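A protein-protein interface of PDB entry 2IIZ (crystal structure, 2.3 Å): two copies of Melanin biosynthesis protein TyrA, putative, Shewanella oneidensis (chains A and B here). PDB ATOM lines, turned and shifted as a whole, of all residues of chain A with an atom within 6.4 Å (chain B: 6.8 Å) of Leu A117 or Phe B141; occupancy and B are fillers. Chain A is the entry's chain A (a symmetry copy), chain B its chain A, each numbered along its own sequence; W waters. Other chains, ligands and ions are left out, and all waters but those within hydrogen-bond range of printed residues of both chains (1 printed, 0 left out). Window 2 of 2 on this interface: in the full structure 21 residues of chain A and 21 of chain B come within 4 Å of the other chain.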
ATOM      1  N   TYR A  47      28.665  30.401  11.263  1.00  0.00           N
ATOM      2  CA  TYR A  47      27.807  29.777  12.260  1.00  0.00           C
ATOM      3  C   TYR A  47      26.788  30.790  12.750  1.00  0.00           C
ATOM      4  O   TYR A  47      25.595  30.512  12.752  1.00  0.00           O
ATOM      5  CB  TYR A  47      28.705  29.263  13.389  1.00  0.00           C
ATOM      6  CG  TYR A  47      28.061  28.698  14.631  1.00  0.00           C
ATOM      7  CD1 TYR A  47      27.213  27.597  14.585  1.00  0.00           C
ATOM      8  CD2 TYR A  47      28.333  29.268  15.880  1.00  0.00           C
ATOM      9  CE1 TYR A  47      26.637  27.091  15.767  1.00  0.00           C
ATOM     10  CE2 TYR A  47      27.772  28.780  17.044  1.00  0.00           C
ATOM     11  CZ  TYR A  47      26.930  27.699  16.996  1.00  0.00           C
ATOM     12  OH  TYR A  47      26.396  27.251  18.193  1.00  0.00           O
ATOM     13  N   TYR A  55      17.458  29.543  14.723  1.00  0.00           N
ATOM     14  CA  TYR A  55      16.751  30.128  15.861  1.00  0.00           C
ATOM     15  C   TYR A  55      15.923  31.323  15.406  1.00  0.00           C
ATOM     16  O   TYR A  55      15.975  32.387  16.005  1.00  0.00           O
ATOM     17  CB  TYR A  55      17.747  30.530  16.962  1.00  0.00           C
ATOM     18  CG  TYR A  55      18.514  29.349  17.564  1.00  0.00           C
ATOM     19  CD1 TYR A  55      17.844  28.291  18.173  1.00  0.00           C
ATOM     20  CD2 TYR A  55      19.902  29.295  17.528  1.00  0.00           C
ATOM     21  CE1 TYR A  55      18.543  27.200  18.731  1.00  0.00           C
ATOM     22  CE2 TYR A  55      20.603  28.212  18.083  1.00  0.00           C
ATOM     23  CZ  TYR A  55      19.925  27.170  18.679  1.00  0.00           C
ATOM     24  OH  TYR A  55      20.645  26.101  19.223  1.00  0.00           O
ATOM     25  N   ARG A 111      15.776  35.037  23.556  1.00  0.00           N
ATOM     26  CA  ARG A 111      15.951  33.981  24.546  1.00  0.00           C
ATOM     27  C   ARG A 111      17.379  34.049  25.024  1.00  0.00           C
ATOM     28  O   ARG A 111      18.316  34.133  24.228  1.00  0.00           O
ATOM     29  CB  ARG A 111      15.687  32.597  23.947  1.00  0.00           C
ATOM     30  CG  ARG A 111      14.230  32.325  23.663  1.00  0.00           C
ATOM     31  CD  ARG A 111      13.967  30.920  23.186  1.00  0.00           C
ATOM     32  NE  ARG A 111      14.433  29.908  24.141  1.00  0.00           N
ATOM     33  CZ  ARG A 111      14.112  28.615  24.065  1.00  0.00           C
ATOM     34  NH1 ARG A 111      13.326  28.170  23.093  1.00  0.00           N
ATOM     35  NH2 ARG A 111      14.569  27.753  24.966  1.00  0.00           N
ATOM     36  N   TYR A 112      17.528  34.003  26.335  1.00  0.00           N
ATOM     37  CA  TYR A 112      18.817  34.143  27.007  1.00  0.00           C
ATOM     38  C   TYR A 112      19.515  32.819  27.072  1.00  0.00           C
ATOM     39  O   TYR A 112      20.724  32.762  27.027  1.00  0.00           O
ATOM     40  CB  TYR A 112      18.533  34.639  28.413  1.00  0.00           C
ATOM     41  CG  TYR A 112      19.675  34.889  29.371  1.00  0.00           C
ATOM     42  CD1 TYR A 112      20.272  33.833  30.069  1.00  0.00           C
ATOM     43  CD2 TYR A 112      20.134  36.189  29.616  1.00  0.00           C
ATOM     44  CE1 TYR A 112      21.310  34.066  30.973  1.00  0.00           C
ATOM     45  CE2 TYR A 112      21.180  36.441  30.526  1.00  0.00           C
ATOM     46  CZ  TYR A 112      21.767  35.376  31.204  1.00  0.00           C
ATOM     47  OH  TYR A 112      22.806  35.589  32.111  1.00  0.00           O
ATOM     48  N   ASP A 113      18.742  31.748  27.185  1.00  0.00           N
ATOM     49  CA  ASP A 113      19.333  30.435  27.306  1.00  0.00           C
ATOM     50  C   ASP A 113      20.082  30.079  26.021  1.00  0.00           C
ATOM     51  O   ASP A 113      21.150  29.460  26.050  1.00  0.00           O
ATOM     52  CB  ASP A 113      18.299  29.364  27.758  1.00  0.00           C
ATOM     53  CG  ASP A 113      17.038  29.254  26.860  1.00  0.00           C
ATOM     54  OD1 ASP A 113      16.866  29.992  25.845  1.00  0.00           O
ATOM     55  OD2 ASP A 113      16.188  28.372  27.206  1.00  0.00           O
ATOM     56  N   ILE A 114      19.521  30.491  24.895  1.00  0.00           N
ATOM     57  CA  ILE A 114      20.124  30.215  23.616  1.00  0.00           C
ATOM     58  C   ILE A 114      21.418  30.987  23.415  1.00  0.00           C
ATOM     59  O   ILE A 114      22.338  30.488  22.787  1.00  0.00           O
ATOM     60  CB  ILE A 114      19.125  30.523  22.494  1.00  0.00           C
ATOM     61  CG1 ILE A 114      18.095  29.400  22.439  1.00  0.00           C
ATOM     62  CG2 ILE A 114      19.821  30.680  21.166  1.00  0.00           C
ATOM     63  CD1 ILE A 114      16.933  29.718  21.549  1.00  0.00           C
ATOM     64  N   LEU A 115      21.492  32.204  23.943  1.00  0.00           N
ATOM     65  CA  LEU A 115      22.746  32.989  23.878  1.00  0.00           C
ATOM     66  C   LEU A 115      23.837  32.389  24.775  1.00  0.00           C
ATOM     67  O   LEU A 115      25.025  32.393  24.436  1.00  0.00           O
ATOM     68  CB  LEU A 115      22.491  34.425  24.303  1.00  0.00           C
ATOM     69  CG  LEU A 115      21.591  35.268  23.406  1.00  0.00           C
ATOM     70  CD1 LEU A 115      21.198  36.571  24.110  1.00  0.00           C
ATOM     71  CD2 LEU A 115      22.270  35.587  22.091  1.00  0.00           C
ATOM     72  N   HIS A 116      23.430  31.873  25.930  1.00  0.00           N
ATOM     73  CA  HIS A 116      24.379  31.229  26.814  1.00  0.00           C
ATOM     74  C   HIS A 116      24.988  30.073  26.054  1.00  0.00           C
ATOM     75  O   HIS A 116      26.197  29.923  26.025  1.00  0.00           O
ATOM     76  CB  HIS A 116      23.701  30.744  28.076  1.00  0.00           C
ATOM     77  CG  HIS A 116      24.656  30.275  29.125  1.00  0.00           C
ATOM     78  ND1 HIS A 116      25.205  31.122  30.063  1.00  0.00           N
ATOM     79  CD2 HIS A 116      25.158  29.043  29.384  1.00  0.00           C
ATOM     80  CE1 HIS A 116      26.005  30.430  30.855  1.00  0.00           C
ATOM     81  NE2 HIS A 116      25.992  29.168  30.464  1.00  0.00           N
ATOM     82  N   LEU A 117      24.136  29.262  25.428  1.00  0.00           N
ATOM     83  CA  LEU A 117      24.583  28.093  24.673  1.00  0.00           C
ATOM     84  C   LEU A 117      25.519  28.508  23.532  1.00  0.00           C
ATOM     85  O   LEU A 117      26.617  27.960  23.367  1.00  0.00           O
ATOM     86  CB  LEU A 117      23.360  27.351  24.138  1.00  0.00           C
ATOM     87  CG  LEU A 117      23.534  26.078  23.295  1.00  0.00           C
ATOM     88  CD1 LEU A 117      22.387  25.116  23.547  1.00  0.00           C
ATOM     89  CD2 LEU A 117      23.611  26.364  21.808  1.00  0.00           C
ATOM     90  N   VAL A 118      25.085  29.485  22.741  1.00  0.00           N
ATOM     91  CA  VAL A 118      25.862  29.914  21.590  1.00  0.00           C
ATOM     92  C   VAL A 118      27.220  30.466  21.979  1.00  0.00           C
ATOM     93  O   VAL A 118      28.215  30.105  21.359  1.00  0.00           O
ATOM     94  CB  VAL A 118      25.079  30.925  20.746  1.00  0.00           C
ATOM     95  CG1 VAL A 118      25.978  31.647  19.772  1.00  0.00           C
ATOM     96  CG2 VAL A 118      23.962  30.200  20.009  1.00  0.00           C
ATOM     97  N   ALA A 119      27.252  31.336  22.993  1.00  0.00           N
ATOM     98  CA  ALA A 119      28.495  31.869  23.565  1.00  0.00           C
ATOM     99  C   ALA A 119      29.461  30.757  23.985  1.00  0.00           C
ATOM    100  O   ALA A 119      30.613  30.727  23.571  1.00  0.00           O
ATOM    101  CB  ALA A 119      28.182  32.765  24.795  1.00  0.00           C
ATOM    102  N   ASN A 120      28.984  29.846  24.825  1.00  0.00           N
ATOM    103  CA  ASN A 120      29.777  28.679  25.186  1.00  0.00           C
ATOM    104  C   ASN A 120      30.334  28.085  23.884  1.00  0.00           C
ATOM    105  O   ASN A 120      31.543  27.881  23.753  1.00  0.00           O
ATOM    106  CB  ASN A 120      28.938  27.634  25.956  1.00  0.00           C
ATOM    107  CG  ASN A 120      28.778  27.955  27.456  1.00  0.00           C
ATOM    108  OD1 ASN A 120      29.535  28.723  28.045  1.00  0.00           O
ATOM    109  ND2 ASN A 120      27.778  27.338  28.074  1.00  0.00           N
ATOM    110  N   GLU A 121      29.459  27.823  22.914  1.00  0.00           N
ATOM    111  CA  GLU A 121      29.912  27.191  21.669  1.00  0.00           C
ATOM    112  C   GLU A 121      30.985  27.997  20.944  1.00  0.00           C
ATOM    113  O   GLU A 121      31.999  27.448  20.518  1.00  0.00           O
ATOM    114  CB  GLU A 121      28.746  26.861  20.728  1.00  0.00           C
ATOM    115  CG  GLU A 121      28.395  25.366  20.723  1.00  0.00           C
ATOM    116  CD  GLU A 121      29.616  24.481  20.385  1.00  0.00           C
ATOM    117  OE1 GLU A 121      30.490  24.935  19.598  1.00  0.00           O
ATOM    118  OE2 GLU A 121      29.704  23.341  20.904  1.00  0.00           O
ATOM    119  N   ILE A 122      30.769  29.296  20.806  1.00  0.00           N
ATOM    120  CA  ILE A 122      31.732  30.130  20.104  1.00  0.00           C
ATOM    121  C   ILE A 122      33.092  30.159  20.804  1.00  0.00           C
ATOM    122  O   ILE A 122      34.137  30.116  20.150  1.00  0.00           O
ATOM    123  CB  ILE A 122      31.160  31.545  19.866  1.00  0.00           C
ATOM    124  CG1 ILE A 122      30.230  31.474  18.650  1.00  0.00           C
ATOM    125  CG2 ILE A 122      32.262  32.558  19.616  1.00  0.00           C
ATOM    126  CD1 ILE A 122      29.359  32.657  18.465  1.00  0.00           C
ATOM    127  N   LEU B  20      11.574  31.815  34.536  1.00  0.00           N
ATOM    128  CA  LEU B  20      12.625  31.971  33.538  1.00  0.00           C
ATOM    129  C   LEU B  20      13.908  32.641  34.056  1.00  0.00           C
ATOM    130  O   LEU B  20      14.975  32.437  33.481  1.00  0.00           O
ATOM    131  CB  LEU B  20      12.112  32.758  32.331  1.00  0.00           C
ATOM    132  CG  LEU B  20      10.920  32.137  31.592  1.00  0.00           C
ATOM    133  CD1 LEU B  20      10.393  33.043  30.448  1.00  0.00           C
ATOM    134  CD2 LEU B  20      11.285  30.784  31.048  1.00  0.00           C
ATOM    135  N   PHE B 139      19.074  31.436  35.343  1.00  0.00           N
ATOM    136  CA  PHE B 139      18.221  31.368  34.174  1.00  0.00           C
ATOM    137  C   PHE B 139      17.773  29.939  33.896  1.00  0.00           C
ATOM    138  O   PHE B 139      18.554  29.006  34.074  1.00  0.00           O
ATOM    139  CB  PHE B 139      18.951  31.931  32.974  1.00  0.00           C
ATOM    140  CG  PHE B 139      20.205  31.185  32.617  1.00  0.00           C
ATOM    141  CD1 PHE B 139      21.395  31.437  33.282  1.00  0.00           C
ATOM    142  CD2 PHE B 139      20.196  30.234  31.606  1.00  0.00           C
ATOM    143  CE1 PHE B 139      22.562  30.751  32.952  1.00  0.00           C
ATOM    144  CE2 PHE B 139      21.367  29.542  31.263  1.00  0.00           C
ATOM    145  CZ  PHE B 139      22.547  29.805  31.939  1.00  0.00           C
ATOM    146  N   ARG B 140      16.521  29.783  33.474  1.00  0.00           N
ATOM    147  CA  ARG B 140      16.046  28.519  32.919  1.00  0.00           C
ATOM    148  C   ARG B 140      16.837  28.163  31.665  1.00  0.00           C
ATOM    149  O   ARG B 140      17.021  29.006  30.793  1.00  0.00           O
ATOM    150  CB  ARG B 140      14.573  28.602  32.550  1.00  0.00           C
ATOM    151  CG  ARG B 140      14.010  27.296  31.996  1.00  0.00           C
ATOM    152  CD  ARG B 140      12.503  27.350  31.784  1.00  0.00           C
ATOM    153  NE  ARG B 140      11.777  27.354  33.052  1.00  0.00           N
ATOM    154  CZ  ARG B 140      10.451  27.455  33.177  1.00  0.00           C
ATOM    155  NH1 ARG B 140       9.676  27.563  32.107  1.00  0.00           N
ATOM    156  NH2 ARG B 140       9.890  27.448  34.386  1.00  0.00           N
ATOM    157  N   PHE B 141      17.304  26.917  31.579  1.00  0.00           N
ATOM    158  CA  PHE B 141      18.039  26.467  30.405  1.00  0.00           C
ATOM    159  C   PHE B 141      17.179  25.430  29.685  1.00  0.00           C
ATOM    160  O   PHE B 141      16.872  24.371  30.227  1.00  0.00           O
ATOM    161  CB  PHE B 141      19.395  25.878  30.803  1.00  0.00           C
ATOM    162  CG  PHE B 141      20.271  25.519  29.629  1.00  0.00           C
ATOM    163  CD1 PHE B 141      20.774  26.507  28.791  1.00  0.00           C
ATOM    164  CD2 PHE B 141      20.592  24.191  29.360  1.00  0.00           C
ATOM    165  CE1 PHE B 141      21.570  26.191  27.725  1.00  0.00           C
ATOM    166  CE2 PHE B 141      21.402  23.855  28.283  1.00  0.00           C
ATOM    167  CZ  PHE B 141      21.892  24.861  27.461  1.00  0.00           C
ATOM    168  N   MET B 142      16.792  25.750  28.459  1.00  0.00           N
ATOM    169  CA  MET B 142      15.949  24.856  27.640  1.00  0.00           C
ATOM    170  C   MET B 142      14.629  24.527  28.391  1.00  0.00           C
ATOM    171  O   MET B 142      14.055  25.427  28.989  1.00  0.00           O
ATOM    172  CB  MET B 142      16.755  23.612  27.219  1.00  0.00           C
ATOM    173  CG  MET B 142      18.054  23.955  26.486  1.00  0.00           C
ATOM    174  SD  MET B 142      17.859  25.194  24.943  1.00  0.00           S
ATOM    175  CE  MET B 142      17.869  26.726  25.681  1.00  0.00           C
ATOM    176  N   ASP B 143      14.171  23.269  28.356  1.00  0.00           N
ATOM    177  CA  ASP B 143      12.972  22.840  29.100  1.00  0.00           C
ATOM    178  C   ASP B 143      13.330  22.446  30.521  1.00  0.00           C
ATOM    179  O   ASP B 143      13.295  21.268  30.891  1.00  0.00           O
ATOM    180  CB  ASP B 143      12.201  21.693  28.394  1.00  0.00           C
ATOM    181  CG  ASP B 143      13.107  20.653  27.738  1.00  0.00           C
ATOM    182  OD1 ASP B 143      14.282  20.970  27.424  1.00  0.00           O
ATOM    183  OD2 ASP B 143      12.622  19.511  27.529  1.00  0.00           O
ATOM    184  N   SER B 144      13.682  23.457  31.313  1.00  0.00           N
ATOM    185  CA  SER B 144      14.123  23.259  32.695  1.00  0.00           C
ATOM    186  C   SER B 144      15.255  22.238  32.849  1.00  0.00           C
ATOM    187  O   SER B 144      15.176  21.311  33.671  1.00  0.00           O
ATOM    188  CB  SER B 144      12.943  22.883  33.574  1.00  0.00           C
ATOM    189  OG  SER B 144      11.897  23.812  33.368  1.00  0.00           O
ATOM    190  N   ARG B 145      16.312  22.423  32.063  1.00  0.00           N
ATOM    191  CA  ARG B 145      17.483  21.564  32.159  1.00  0.00           C
ATOM    192  C   ARG B 145      18.650  22.285  32.897  1.00  0.00           C
ATOM    193  O   ARG B 145      18.783  23.526  32.898  1.00  0.00           O
ATOM    194  CB  ARG B 145      17.870  21.021  30.763  1.00  0.00           C
ATOM    195  CG  ARG B 145      16.631  20.661  29.892  1.00  0.00           C
ATOM    196  CD  ARG B 145      16.935  20.049  28.520  1.00  0.00           C
ATOM    197  NE  ARG B 145      17.146  18.616  28.663  1.00  0.00           N
ATOM    198  CZ  ARG B 145      16.341  17.632  28.258  1.00  0.00           C
ATOM    199  NH1 ARG B 145      15.198  17.840  27.643  1.00  0.00           N
ATOM    200  NH2 ARG B 145      16.714  16.392  28.492  1.00  0.00           N
ATOM    201  N   ASP B 146      19.480  21.476  33.543  1.00  0.00           N
ATOM    202  CA  ASP B 146      20.753  21.914  34.087  1.00  0.00           C
ATOM    203  C   ASP B 146      21.654  22.001  32.886  1.00  0.00           C
ATOM    204  O   ASP B 146      21.341  21.421  31.840  1.00  0.00           O
ATOM    205  CB  ASP B 146      21.269  20.875  35.093  1.00  0.00           C
ATOM    206  CG  ASP B 146      22.675  21.180  35.607  1.00  0.00           C
ATOM    207  OD1 ASP B 146      22.816  21.991  36.543  1.00  0.00           O
ATOM    208  OD2 ASP B 146      23.638  20.588  35.069  1.00  0.00           O
ATOM    209  N   LEU B 147      22.761  22.716  33.005  1.00  0.00           N
ATOM    210  CA  LEU B 147      23.642  22.908  31.846  1.00  0.00           C
ATOM    211  C   LEU B 147      24.316  21.606  31.397  1.00  0.00           C
ATOM    212  O   LEU B 147      24.894  21.565  30.307  1.00  0.00           O
ATOM    213  CB  LEU B 147      24.684  23.977  32.139  1.00  0.00           C
ATOM    214  CG  LEU B 147      24.127  25.405  32.229  1.00  0.00           C
ATOM    215  CD1 LEU B 147      25.069  26.254  33.015  1.00  0.00           C
ATOM    216  CD2 LEU B 147      23.912  26.015  30.835  1.00  0.00           C
ATOM    217  N   THR B 148      24.233  20.557  32.232  1.00  0.00           N
ATOM    218  CA  THR B 148      24.612  19.196  31.827  1.00  0.00           C
ATOM    219  C   THR B 148      23.737  18.632  30.688  1.00  0.00           C
ATOM    220  O   THR B 148      24.117  17.663  30.032  1.00  0.00           O
ATOM    221  CB  THR B 148      24.589  18.206  33.022  1.00  0.00           C
ATOM    222  OG1 THR B 148      23.351  18.307  33.746  1.00  0.00           O
ATOM    223  CG2 THR B 148      25.689  18.537  33.968  1.00  0.00           C
ATOM    224  N   GLY B 149      22.572  19.247  30.457  1.00  0.00           N
ATOM    225  CA  GLY B 149      21.642  18.822  29.412  1.00  0.00           C
ATOM    226  C   GLY B 149      20.562  17.878  29.921  1.00  0.00           C
ATOM    227  O   GLY B 149      19.746  17.412  29.125  1.00  0.00           O
ATOM    228  N   PHE B 150      20.560  17.598  31.233  1.00  0.00           N
ATOM    229  CA  PHE B 150      19.543  16.768  31.908  1.00  0.00           C
ATOM    230  C   PHE B 150      18.510  17.622  32.626  1.00  0.00           C
ATOM    231  O   PHE B 150      18.861  18.650  33.207  1.00  0.00           O
ATOM    232  CB  PHE B 150      20.209  15.870  32.960  1.00  0.00           C
ATOM    233  CG  PHE B 150      20.962  14.710  32.371  1.00  0.00           C
ATOM    234  CD1 PHE B 150      22.193  14.910  31.758  1.00  0.00           C
ATOM    235  CD2 PHE B 150      20.439  13.416  32.427  1.00  0.00           C
ATOM    236  CE1 PHE B 150      22.887  13.856  31.209  1.00  0.00           C
ATOM    237  CE2 PHE B 150      21.140  12.350  31.871  1.00  0.00           C
ATOM    238  CZ  PHE B 150      22.359  12.568  31.270  1.00  0.00           C
ATOM    239  N   MET B 246      18.652  26.803  39.985  1.00  0.00           N
ATOM    240  CA  MET B 246      18.645  27.234  38.587  1.00  0.00           C
ATOM    241  C   MET B 246      20.058  27.292  38.027  1.00  0.00           C
ATOM    242  O   MET B 246      20.994  27.483  38.787  1.00  0.00           O
ATOM    243  CB  MET B 246      18.019  28.601  38.493  1.00  0.00           C
ATOM    244  CG  MET B 246      16.593  28.588  38.997  1.00  0.00           C
ATOM    245  SD  MET B 246      15.548  30.084  38.572  1.00  0.00           S
ATOM    246  CE  MET B 246      15.691  30.049  36.632  1.00  0.00           C
ATOM    247  N   PRO B 247      20.230  27.119  36.690  1.00  0.00           N
ATOM    248  CA  PRO B 247      21.535  27.387  36.091  1.00  0.00           C
ATOM    249  C   PRO B 247      21.936  28.825  36.359  1.00  0.00           C
ATOM    250  O   PRO B 247      21.056  29.646  36.591  1.00  0.00           O
ATOM    251  CB  PRO B 247      21.278  27.201  34.577  1.00  0.00           C
ATOM    252  CG  PRO B 247      20.132  26.261  34.527  1.00  0.00           C
ATOM    253  CD  PRO B 247      19.264  26.658  35.683  1.00  0.00           C
HETATM  254  O   HOH W   1      13.860  28.219  28.756  1.00  0.00           O
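O of Leu B20 lies within hydrogen-bond range of N of Arg B140 (3.1 Å).
The backbone NH of Phe B139 sits at hydrogen-bond distance from the backbone carbonyl oxygen of Pro B247 (2.9 Å).
NH2 of Arg A111 is in salt-bridge range of OD2 of Asp A113 (2.8 Å).
The backbone NH (N) of Met B142 lies close to the side-chain carboxylate (OD2) of Asp A113.
Met B142 touches Arg A111.
Tyr A112 touches Phe B139 (CE1 to CG, 3.5 Å).
Arg B140 touches Asp A113.
Asp A113 touches Phe B141 (O to CE1, 3.7 Å).
Phe B139 touches His A116 (CZ to ND1, 3.5 Å).
His A116 touches Leu B147.
Leu A117 touches Phe B141.
Water W1 lies within hydrogen-bond range of OD2 of Asp A113 and O of Met B142.
Of the 15 printed residues of chain B, 5 touch a printed residue of chain A.
Printed residues of chain B that touch a printed residue of chain A: Phe B139, Arg B140, Phe B141, Met B142 and Leu B147.
Hydrophobic or aromatic side chains of chain B within 4 Å of the printed part of chain A: Phe B139, Phe B141, Met B142 and Leu B147.
Of the 14 printed residues of chain A, 5 touch a printed residue of chain B.
Of the printed residues of chain B, Leu A117 touches Phe B141.
Phe B141 touches just these residues of chain A: Asp A113 (3.7 Å) and Leu A117 (3.95 Å).
Of the printed residues of chain A, Met B142 touches Arg A111 (3.5 Å) and Asp A113 (2.8 Å).
Of the printed residues of chain B, Arg A111 touches Met B142 (3.5 Å).
Of the printed residues of chain A, Leu B147 touches His A116.
The nearest residue of chain B that does not touch Leu A117 is Met B142 (4.7 Å).
No position is printed for both chains.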
